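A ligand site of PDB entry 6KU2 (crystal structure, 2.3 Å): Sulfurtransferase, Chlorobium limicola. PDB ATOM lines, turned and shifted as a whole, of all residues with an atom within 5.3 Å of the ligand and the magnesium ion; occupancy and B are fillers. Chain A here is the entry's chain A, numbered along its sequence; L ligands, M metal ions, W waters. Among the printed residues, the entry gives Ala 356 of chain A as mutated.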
ATOM      1  N   TYR A 191      11.166  -6.734   5.353  1.00  0.00           N
ATOM      2  CA  TYR A 191      11.618  -6.798   3.960  1.00  0.00           C
ATOM      3  C   TYR A 191      12.664  -7.885   3.876  1.00  0.00           C
ATOM      4  O   TYR A 191      13.771  -7.726   4.387  1.00  0.00           O
ATOM      5  CB  TYR A 191      12.247  -5.459   3.532  1.00  0.00           C
ATOM      6  CG  TYR A 191      12.990  -5.507   2.200  1.00  0.00           C
ATOM      7  CD1 TYR A 191      12.430  -6.083   1.077  1.00  0.00           C
ATOM      8  CD2 TYR A 191      14.250  -4.961   2.059  1.00  0.00           C
ATOM      9  CE1 TYR A 191      13.086  -6.080  -0.138  1.00  0.00           C
ATOM     10  CE2 TYR A 191      14.910  -4.967   0.843  1.00  0.00           C
ATOM     11  CZ  TYR A 191      14.318  -5.503  -0.259  1.00  0.00           C
ATOM     12  OH  TYR A 191      14.960  -5.495  -1.475  1.00  0.00           O
ATOM     13  N   THR A 210       7.408  -7.227   2.999  1.00  0.00           N
ATOM     14  CA  THR A 210       6.907  -6.058   2.219  1.00  0.00           C
ATOM     15  C   THR A 210       6.792  -6.410   0.736  1.00  0.00           C
ATOM     16  O   THR A 210       5.974  -5.818   0.084  1.00  0.00           O
ATOM     17  CB  THR A 210       7.727  -4.791   2.478  1.00  0.00           C
ATOM     18  OG1 THR A 210       9.074  -5.072   2.181  1.00  0.00           O
ATOM     19  CG2 THR A 210       7.611  -4.284   3.890  1.00  0.00           C
ATOM     20  N   GLU A 214       4.460  -5.093  -2.481  1.00  0.00           N
ATOM     21  CA  GLU A 214       5.087  -4.231  -3.458  1.00  0.00           C
ATOM     22  C   GLU A 214       6.006  -5.020  -4.374  1.00  0.00           C
ATOM     23  O   GLU A 214       6.487  -6.115  -4.014  1.00  0.00           O
ATOM     24  CB  GLU A 214       5.820  -3.066  -2.786  1.00  0.00           C
ATOM     25  CG  GLU A 214       6.779  -3.408  -1.688  1.00  0.00           C
ATOM     26  CD  GLU A 214       7.488  -2.194  -1.064  1.00  0.00           C
ATOM     27  OE1 GLU A 214       7.027  -1.050  -1.232  1.00  0.00           O
ATOM     28  OE2 GLU A 214       8.526  -2.385  -0.383  1.00  0.00           O
ATOM     29  N   THR A 218       9.241  -2.250  -9.839  1.00  0.00           N
ATOM     30  CA  THR A 218       8.893  -0.819  -9.793  1.00  0.00           C
ATOM     31  C   THR A 218       9.043  -0.202  -8.403  1.00  0.00           C
ATOM     32  O   THR A 218       8.933   1.000  -8.274  1.00  0.00           O
ATOM     33  CB  THR A 218       7.411  -0.628 -10.165  1.00  0.00           C
ATOM     34  OG1 THR A 218       6.631  -1.481  -9.339  1.00  0.00           O
ATOM     35  CG2 THR A 218       7.168  -0.960 -11.653  1.00  0.00           C
ATOM     36  N   TRP A 219       9.234  -1.033  -7.386  1.00  0.00           N
ATOM     37  CA  TRP A 219       9.035  -0.639  -5.980  1.00  0.00           C
ATOM     38  C   TRP A 219       7.763   0.184  -5.736  1.00  0.00           C
ATOM     39  O   TRP A 219       7.669   1.044  -4.845  1.00  0.00           O
ATOM     40  CB  TRP A 219      10.301  -0.008  -5.398  1.00  0.00           C
ATOM     41  CG  TRP A 219      11.493  -0.913  -5.439  1.00  0.00           C
ATOM     42  CD1 TRP A 219      12.640  -0.647  -6.048  1.00  0.00           C
ATOM     43  CD2 TRP A 219      11.658  -2.197  -4.840  1.00  0.00           C
ATOM     44  NE1 TRP A 219      13.535  -1.664  -5.889  1.00  0.00           N
ATOM     45  CE2 TRP A 219      12.948  -2.645  -5.155  1.00  0.00           C
ATOM     46  CE3 TRP A 219      10.844  -3.029  -4.056  1.00  0.00           C
ATOM     47  CZ2 TRP A 219      13.442  -3.847  -4.736  1.00  0.00           C
ATOM     48  CZ3 TRP A 219      11.344  -4.239  -3.647  1.00  0.00           C
ATOM     49  CH2 TRP A 219      12.626  -4.633  -3.988  1.00  0.00           C
ATOM     50  N   ASN A 220       6.741  -0.152  -6.471  1.00  0.00           N
ATOM     51  CA  ASN A 220       5.417   0.419  -6.256  1.00  0.00           C
ATOM     52  C   ASN A 220       4.503  -0.688  -5.785  1.00  0.00           C
ATOM     53  O   ASN A 220       4.844  -1.887  -5.914  1.00  0.00           O
ATOM     54  CB  ASN A 220       4.904   1.071  -7.561  1.00  0.00           C
ATOM     55  CG  ASN A 220       5.496   2.469  -7.803  1.00  0.00           C
ATOM     56  OD1 ASN A 220       6.348   2.978  -7.027  1.00  0.00           O
ATOM     57  ND2 ASN A 220       5.040   3.099  -8.890  1.00  0.00           N
ATOM     58  N   ARG A 221       3.364  -0.291  -5.212  1.00  0.00           N
ATOM     59  CA  ARG A 221       2.315  -1.242  -4.851  1.00  0.00           C
ATOM     60  C   ARG A 221       1.994  -2.202  -6.012  1.00  0.00           C
ATOM     61  O   ARG A 221       2.038  -1.868  -7.204  1.00  0.00           O
ATOM     62  CB  ARG A 221       1.021  -0.518  -4.439  1.00  0.00           C
ATOM     63  CG  ARG A 221       0.374   0.294  -5.569  1.00  0.00           C
ATOM     64  CD  ARG A 221      -0.432   1.504  -5.103  1.00  0.00           C
ATOM     65  NE  ARG A 221      -1.127   2.098  -6.246  1.00  0.00           N
ATOM     66  CZ  ARG A 221      -0.578   2.960  -7.101  1.00  0.00           C
ATOM     67  NH1 ARG A 221       0.699   3.353  -6.975  1.00  0.00           N
ATOM     68  NH2 ARG A 221      -1.316   3.416  -8.105  1.00  0.00           N
ATOM     69  N   PRO A 258      19.756  -2.738   3.774  1.00  0.00           N
ATOM     70  CA  PRO A 258      19.500  -1.985   5.016  1.00  0.00           C
ATOM     71  C   PRO A 258      18.029  -1.933   5.440  1.00  0.00           C
ATOM     72  O   PRO A 258      17.777  -1.831   6.620  1.00  0.00           O
ATOM     73  CB  PRO A 258      19.993  -0.570   4.672  1.00  0.00           C
ATOM     74  CG  PRO A 258      20.937  -0.750   3.512  1.00  0.00           C
ATOM     75  CD  PRO A 258      20.308  -1.851   2.729  1.00  0.00           C
ATOM     76  N   GLY A 259      17.100  -2.025   4.473  1.00  0.00           N
ATOM     77  CA  GLY A 259      15.669  -1.985   4.708  1.00  0.00           C
ATOM     78  C   GLY A 259      15.135  -3.153   5.475  1.00  0.00           C
ATOM     79  O   GLY A 259      14.086  -3.041   6.166  1.00  0.00           O
ATOM     80  N   SER A 260      15.872  -4.267   5.399  1.00  0.00           N
ATOM     81  CA  SER A 260      15.597  -5.465   6.206  1.00  0.00           C
ATOM     82  C   SER A 260      15.685  -5.170   7.719  1.00  0.00           C
ATOM     83  O   SER A 260      15.083  -5.888   8.524  1.00  0.00           O
ATOM     84  CB  SER A 260      16.581  -6.592   5.835  1.00  0.00           C
ATOM     85  OG  SER A 260      16.366  -7.088   4.513  1.00  0.00           O
ATOM     86  N   ARG A 269       4.556   1.521   5.758  1.00  0.00           N
ATOM     87  CA  ARG A 269       4.409   1.414   4.302  1.00  0.00           C
ATOM     88  C   ARG A 269       3.311   0.449   3.943  1.00  0.00           C
ATOM     89  O   ARG A 269       2.479   0.754   3.080  1.00  0.00           O
ATOM     90  CB  ARG A 269       5.734   1.007   3.640  1.00  0.00           C
ATOM     91  CG  ARG A 269       5.609   0.448   2.220  1.00  0.00           C
ATOM     92  CD  ARG A 269       5.380   1.547   1.203  1.00  0.00           C
ATOM     93  NE  ARG A 269       5.469   1.023  -0.144  1.00  0.00           N
ATOM     94  CZ  ARG A 269       5.164   1.699  -1.256  1.00  0.00           C
ATOM     95  NH1 ARG A 269       5.293   1.103  -2.413  1.00  0.00           N
ATOM     96  NH2 ARG A 269       4.711   2.943  -1.227  1.00  0.00           N
ATOM     97  N   ALA A 356      20.027   5.028  -2.121  1.00  0.00           N
ATOM     98  CA  ALA A 356      19.967   3.571  -2.050  1.00  0.00           C
ATOM     99  C   ALA A 356      20.896   2.972  -3.104  1.00  0.00           C
ATOM    100  O   ALA A 356      21.203   3.639  -4.107  1.00  0.00           O
ATOM    101  CB  ALA A 356      18.551   3.126  -2.313  1.00  0.00           C
ATOM    102  N   TYR A 358      20.322   0.628  -5.349  1.00  0.00           N
ATOM    103  CA  TYR A 358      19.687   0.237  -6.610  1.00  0.00           C
ATOM    104  C   TYR A 358      19.190   1.475  -7.401  1.00  0.00           C
ATOM    105  O   TYR A 358      18.471   1.347  -8.406  1.00  0.00           O
ATOM    106  CB  TYR A 358      18.516  -0.687  -6.312  1.00  0.00           C
ATOM    107  CG  TYR A 358      17.587  -0.190  -5.201  1.00  0.00           C
ATOM    108  CD1 TYR A 358      16.504   0.655  -5.489  1.00  0.00           C
ATOM    109  CD2 TYR A 358      17.764  -0.589  -3.856  1.00  0.00           C
ATOM    110  CE1 TYR A 358      15.617   1.100  -4.480  1.00  0.00           C
ATOM    111  CE2 TYR A 358      16.923  -0.123  -2.849  1.00  0.00           C
ATOM    112  CZ  TYR A 358      15.835   0.722  -3.168  1.00  0.00           C
ATOM    113  OH  TYR A 358      14.966   1.167  -2.198  1.00  0.00           O
ATOM    114  N   ALA A 377      18.202   7.014   3.994  1.00  0.00           N
ATOM    115  CA  ALA A 377      16.933   6.461   3.544  1.00  0.00           C
ATOM    116  C   ALA A 377      16.260   5.482   4.500  1.00  0.00           C
ATOM    117  O   ALA A 377      15.092   5.119   4.321  1.00  0.00           O
ATOM    118  CB  ALA A 377      17.096   5.816   2.202  1.00  0.00           C
ATOM    119  N   TYR A 378      16.996   5.037   5.495  1.00  0.00           N
ATOM    120  CA  TYR A 378      16.507   3.990   6.395  1.00  0.00           C
ATOM    121  C   TYR A 378      16.206   4.492   7.802  1.00  0.00           C
ATOM    122  O   TYR A 378      15.924   3.671   8.667  1.00  0.00           O
ATOM    123  CB  TYR A 378      17.555   2.866   6.388  1.00  0.00           C
ATOM    124  CG  TYR A 378      17.728   2.350   4.983  1.00  0.00           C
ATOM    125  CD1 TYR A 378      16.780   1.530   4.439  1.00  0.00           C
ATOM    126  CD2 TYR A 378      18.791   2.755   4.208  1.00  0.00           C
ATOM    127  CE1 TYR A 378      16.852   1.092   3.162  1.00  0.00           C
ATOM    128  CE2 TYR A 378      18.887   2.330   2.895  1.00  0.00           C
ATOM    129  CZ  TYR A 378      17.919   1.488   2.387  1.00  0.00           C
ATOM    130  OH  TYR A 378      17.985   1.048   1.089  1.00  0.00           O
ATOM    131  N   CYS A 415       9.490   9.716  -1.323  1.00  0.00           N
ATOM    132  CA  CYS A 415      10.857   9.605  -0.935  1.00  0.00           C
ATOM    133  C   CYS A 415      11.483   8.857  -2.097  1.00  0.00           C
ATOM    134  O   CYS A 415      11.177   9.170  -3.195  1.00  0.00           O
ATOM    135  CB  CYS A 415      10.974   8.833   0.344  1.00  0.00           C
ATOM    136  SG  CYS A 415      10.303   7.227   0.244  1.00  0.00           S
ATOM    137  N   GLY A 416      12.389   7.946  -1.831  1.00  0.00           N
ATOM    138  CA  GLY A 416      12.943   7.170  -2.895  1.00  0.00           C
ATOM    139  C   GLY A 416      12.048   6.152  -3.569  1.00  0.00           C
ATOM    140  O   GLY A 416      11.924   6.200  -4.738  1.00  0.00           O
ATOM    141  N   THR A 417      11.384   5.289  -2.810  1.00  0.00           N
ATOM    142  CA  THR A 417      10.490   4.248  -3.314  1.00  0.00           C
ATOM    143  C   THR A 417       9.113   4.286  -2.707  1.00  0.00           C
ATOM    144  O   THR A 417       8.247   3.602  -3.121  1.00  0.00           O
ATOM    145  CB  THR A 417      11.030   2.829  -3.110  1.00  0.00           C
ATOM    146  OG1 THR A 417      11.159   2.571  -1.723  1.00  0.00           O
ATOM    147  CG2 THR A 417      12.329   2.663  -3.775  1.00  0.00           C
ATOM    148  N   GLY A 418       8.943   5.094  -1.701  1.00  0.00           N
ATOM    149  CA  GLY A 418       7.616   5.262  -1.070  1.00  0.00           C
ATOM    150  C   GLY A 418       7.479   4.846   0.394  1.00  0.00           C
ATOM    151  O   GLY A 418       6.419   5.017   0.948  1.00  0.00           O
ATOM    152  N   TRP A 419       8.554   4.337   1.018  1.00  0.00           N
ATOM    153  CA  TRP A 419       8.532   3.920   2.457  1.00  0.00           C
ATOM    154  C   TRP A 419       8.476   5.120   3.426  1.00  0.00           C
ATOM    155  O   TRP A 419       7.596   5.208   4.278  1.00  0.00           O
ATOM    156  CB  TRP A 419       9.748   3.032   2.787  1.00  0.00           C
ATOM    157  CG  TRP A 419       9.617   1.626   2.468  1.00  0.00           C
ATOM    158  CD1 TRP A 419       8.987   1.061   1.398  1.00  0.00           C
ATOM    159  CD2 TRP A 419      10.124   0.547   3.250  1.00  0.00           C
ATOM    160  NE1 TRP A 419       9.088  -0.302   1.461  1.00  0.00           N
ATOM    161  CE2 TRP A 419       9.805  -0.654   2.577  1.00  0.00           C
ATOM    162  CE3 TRP A 419      10.908   0.472   4.431  1.00  0.00           C
ATOM    163  CZ2 TRP A 419      10.207  -1.924   3.057  1.00  0.00           C
ATOM    164  CZ3 TRP A 419      11.308  -0.820   4.918  1.00  0.00           C
ATOM    165  CH2 TRP A 419      10.929  -1.982   4.242  1.00  0.00           C
ATOM    166  N   ARG A 420       9.416   6.051   3.282  1.00  0.00           N
ATOM    167  CA  ARG A 420       9.419   7.242   4.136  1.00  0.00           C
ATOM    168  C   ARG A 420       8.270   8.152   3.756  1.00  0.00           C
ATOM    169  O   ARG A 420       7.699   8.803   4.609  1.00  0.00           O
ATOM    170  CB  ARG A 420      10.710   8.035   3.969  1.00  0.00           C
ATOM    171  CG  ARG A 420      11.937   7.226   4.351  1.00  0.00           C
ATOM    172  CD  ARG A 420      13.184   7.980   3.980  1.00  0.00           C
ATOM    173  NE  ARG A 420      13.516   7.765   2.573  1.00  0.00           N
ATOM    174  CZ  ARG A 420      14.502   8.410   1.951  1.00  0.00           C
ATOM    175  NH1 ARG A 420      15.234   9.324   2.611  1.00  0.00           N
ATOM    176  NH2 ARG A 420      14.803   8.106   0.680  1.00  0.00           N
ATOM    177  N   GLY A 421       7.968   8.229   2.466  1.00  0.00           N
ATOM    178  CA  GLY A 421       6.731   8.897   1.994  1.00  0.00           C
ATOM    179  C   GLY A 421       5.508   8.433   2.750  1.00  0.00           C
ATOM    180  O   GLY A 421       4.676   9.284   3.177  1.00  0.00           O
ATOM    181  N   ASP A 440       3.899   7.213  -5.200  1.00  0.00           N
ATOM    182  CA  ASP A 440       4.554   5.918  -4.954  1.00  0.00           C
ATOM    183  C   ASP A 440       5.921   5.749  -5.621  1.00  0.00           C
ATOM    184  O   ASP A 440       6.898   5.380  -4.971  1.00  0.00           O
ATOM    185  CB  ASP A 440       3.590   4.810  -5.405  1.00  0.00           C
ATOM    186  CG  ASP A 440       3.915   3.471  -4.883  1.00  0.00           C
ATOM    187  OD1 ASP A 440       5.003   3.305  -4.233  1.00  0.00           O
ATOM    188  OD2 ASP A 440       3.096   2.568  -5.156  1.00  0.00           O
ATOM    189  N   GLY A 441       5.995   6.058  -6.913  1.00  0.00           N
ATOM    190  CA  GLY A 441       7.205   5.928  -7.717  1.00  0.00           C
ATOM    191  C   GLY A 441       8.423   6.591  -7.128  1.00  0.00           C
ATOM    192  O   GLY A 441       9.525   6.039  -7.146  1.00  0.00           O
ATOM    193  N   GLY A 442       8.222   7.802  -6.592  1.00  0.00           N
ATOM    194  CA  GLY A 442       9.273   8.539  -5.934  1.00  0.00           C
ATOM    195  C   GLY A 442      10.372   8.842  -6.900  1.00  0.00           C
ATOM    196  O   GLY A 442      10.159   8.875  -8.093  1.00  0.00           O
HETATM  197  C1  LIG L   1      11.701  -0.862  -1.563  1.00  0.00           C
HETATM  198  C2  LIG L   1      13.801  -2.062  -1.645  1.00  0.00           C
HETATM  199  C3  LIG L   1      12.142  -2.488   0.188  1.00  0.00           C
HETATM  200  C4  LIG L   1      13.337  -0.192   0.028  1.00  0.00           C
HETATM  201  C5  LIG L   1      14.778  -0.504   0.603  1.00  0.00           C
HETATM  202  C6  LIG L   1      12.558   0.366   1.207  1.00  0.00           C
HETATM  203  C7  LIG L   1      12.958   1.704   1.542  1.00  0.00           C
HETATM  204  C8  LIG L   1      14.006   3.517   0.915  1.00  0.00           C
HETATM  205  N1  LIG L   1      12.749  -1.390  -0.690  1.00  0.00           N
HETATM  206  O1  LIG L   1      14.849  -1.483   1.422  1.00  0.00           O
HETATM  207  O2  LIG L   1      15.715   0.256   0.223  1.00  0.00           O
HETATM  208  C9  LIG L   1      13.536   2.239   2.723  1.00  0.00           C
HETATM  209  N2  LIG L   1      13.778   3.620   2.382  1.00  0.00           N
HETATM  210  S1  LIG L   1      13.762   5.155  -0.077  1.00  0.00           S
HETATM  211  S2  LIG L   1      11.764   5.761   0.532  1.00  0.00           S
HETATM  212  N3  LIG L   1      12.930   2.689   0.597  1.00  0.00           N
HETATM  213 MG    MG M   1       7.122   3.189  -4.968  1.00  0.00          MG
HETATM  214  O   HOH W   1      17.205  -2.558   1.634  1.00  0.00           O
HETATM  215  O   HOH W   2       8.895   0.876  -2.195  1.00  0.00           O
HETATM  216  O   HOH W   3       9.391   3.258  -6.461  1.00  0.00           O
HETATM  217  O   HOH W   4      16.585  -3.666  -1.974  1.00  0.00           O
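Residues that only touch the ligand: Tyr 191, Glu 214 and Gly 259. Hydrophobic or aromatic side chains that line the ligand: Tyr 191, Trp 219, Tyr 358, Ala 377, Tyr 378 and Trp 419. 13 residues have an atom within 4 Å of the ligand: Tyr 191, Glu 214, Trp 219, Gly 259, Tyr 358, Ala 377, Tyr 378, Cys 415, Gly 416, Thr 417, Gly 418, Trp 419 and Arg 420. The nearest printed residue that does not touch the ligand is Thr 210 (4.5 Å).
S2 of the ligand is bonded to SG of Cys 415 (2.1 Å). The backbone NH of Thr 417 lies close to a sulfur (S2) of the ligand. N3 of the ligand sits at hydrogen-bond distance from OG1 of Thr 417, at 2.9 Å. The side-chain hydroxyl (OH) of Tyr 378 lies within hydrogen-bond range of an oxygen (O2) of the ligand, at 2.6 Å. The side-chain hydroxyl (OH) of Tyr 358 sits at hydrogen-bond distance from an oxygen (O2) of the ligand, 2.7 Å away. N2 of the ligand lies within hydrogen-bond range of O of Ala 377. S2 of the ligand lies close to N of Trp 419, 3.5 Å away. The backbone NH (N) of Arg 420 lies close to a sulfur (S2) of the ligand. NH2 of Arg 420 lies close to S1 of the ligand. A sulfur (S2) of the ligand sits close to the backbone NH (N) of Gly 416 (3.3 Å). A sulfur (S2) of the ligand sits close to the backbone NH (N) of Gly 418, at 3.7 Å.
SG of Cys 415 lies close to N of Thr 417, at 3.8 Å. N of Trp 419 is in hydrogen-bond range of SG of Cys 415. The guanidinium group (NH1) of Arg 221 lies within salt-bridge range of the side-chain carboxylate (OD2) of Asp 440, at 3.1 Å. The backbone NH (N) of Gly 441 lies close to the side-chain amide oxygen (OD1) of Asn 220 (3.1 Å). The side-chain hydroxyl (OG1) of Thr 218 sits close to the backbone NH (N) of Asn 220, 3.2 Å away. The guanidinium group (NH1) of Arg 269 lies close to the backbone carbonyl oxygen (O) of Trp 219, at 3.4 Å. The backbone carbonyl oxygen of Tyr 191 lies within hydrogen-bond range of the side-chain hydroxyl of Ser 260, at 2.7 Å. NH2 of Arg 269 lies within hydrogen-bond range of O of Gly 418 (3.5 Å).
Water W3 lies within hydrogen-bond range of the backbone carbonyl oxygen of Gly 441 (2.9 Å) and the backbone carbonyl oxygen of Thr 218 (2.9 Å). Water W1 lies within hydrogen-bond range of an oxygen (O1) of the ligand (2.6 Å) and the backbone NH (N) of Gly 259 (2.9 Å). Water W2 lies within hydrogen-bond range of the side-chain carboxylate of Glu 214 (2.9 Å) and the side-chain hydroxyl of Thr 417 (2.9 Å).
NH1 of Arg 269 touches the magnesium ion (3.8 Å). Gly 441 touches the magnesium ion. Within 4 Å of the magnesium ion: Trp 219, Asn 220, Arg 269, Thr 417, Asp 440 and Gly 441.
The backbone carbonyl oxygen (O) of Thr 417 binds the magnesium ion (2.2 Å). O of Asp 440 binds the magnesium ion, at 2.2 Å. The magnesium ion is bound by OD1 of Asn 220 (2.2 Å). O of Trp 219 is bound to the magnesium ion (2.2 Å). OD1 of Asp 440 is bound to the magnesium ion, at 2.2 Å. Slightly farther from the magnesium ion lies water W3 (2.7 Å).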
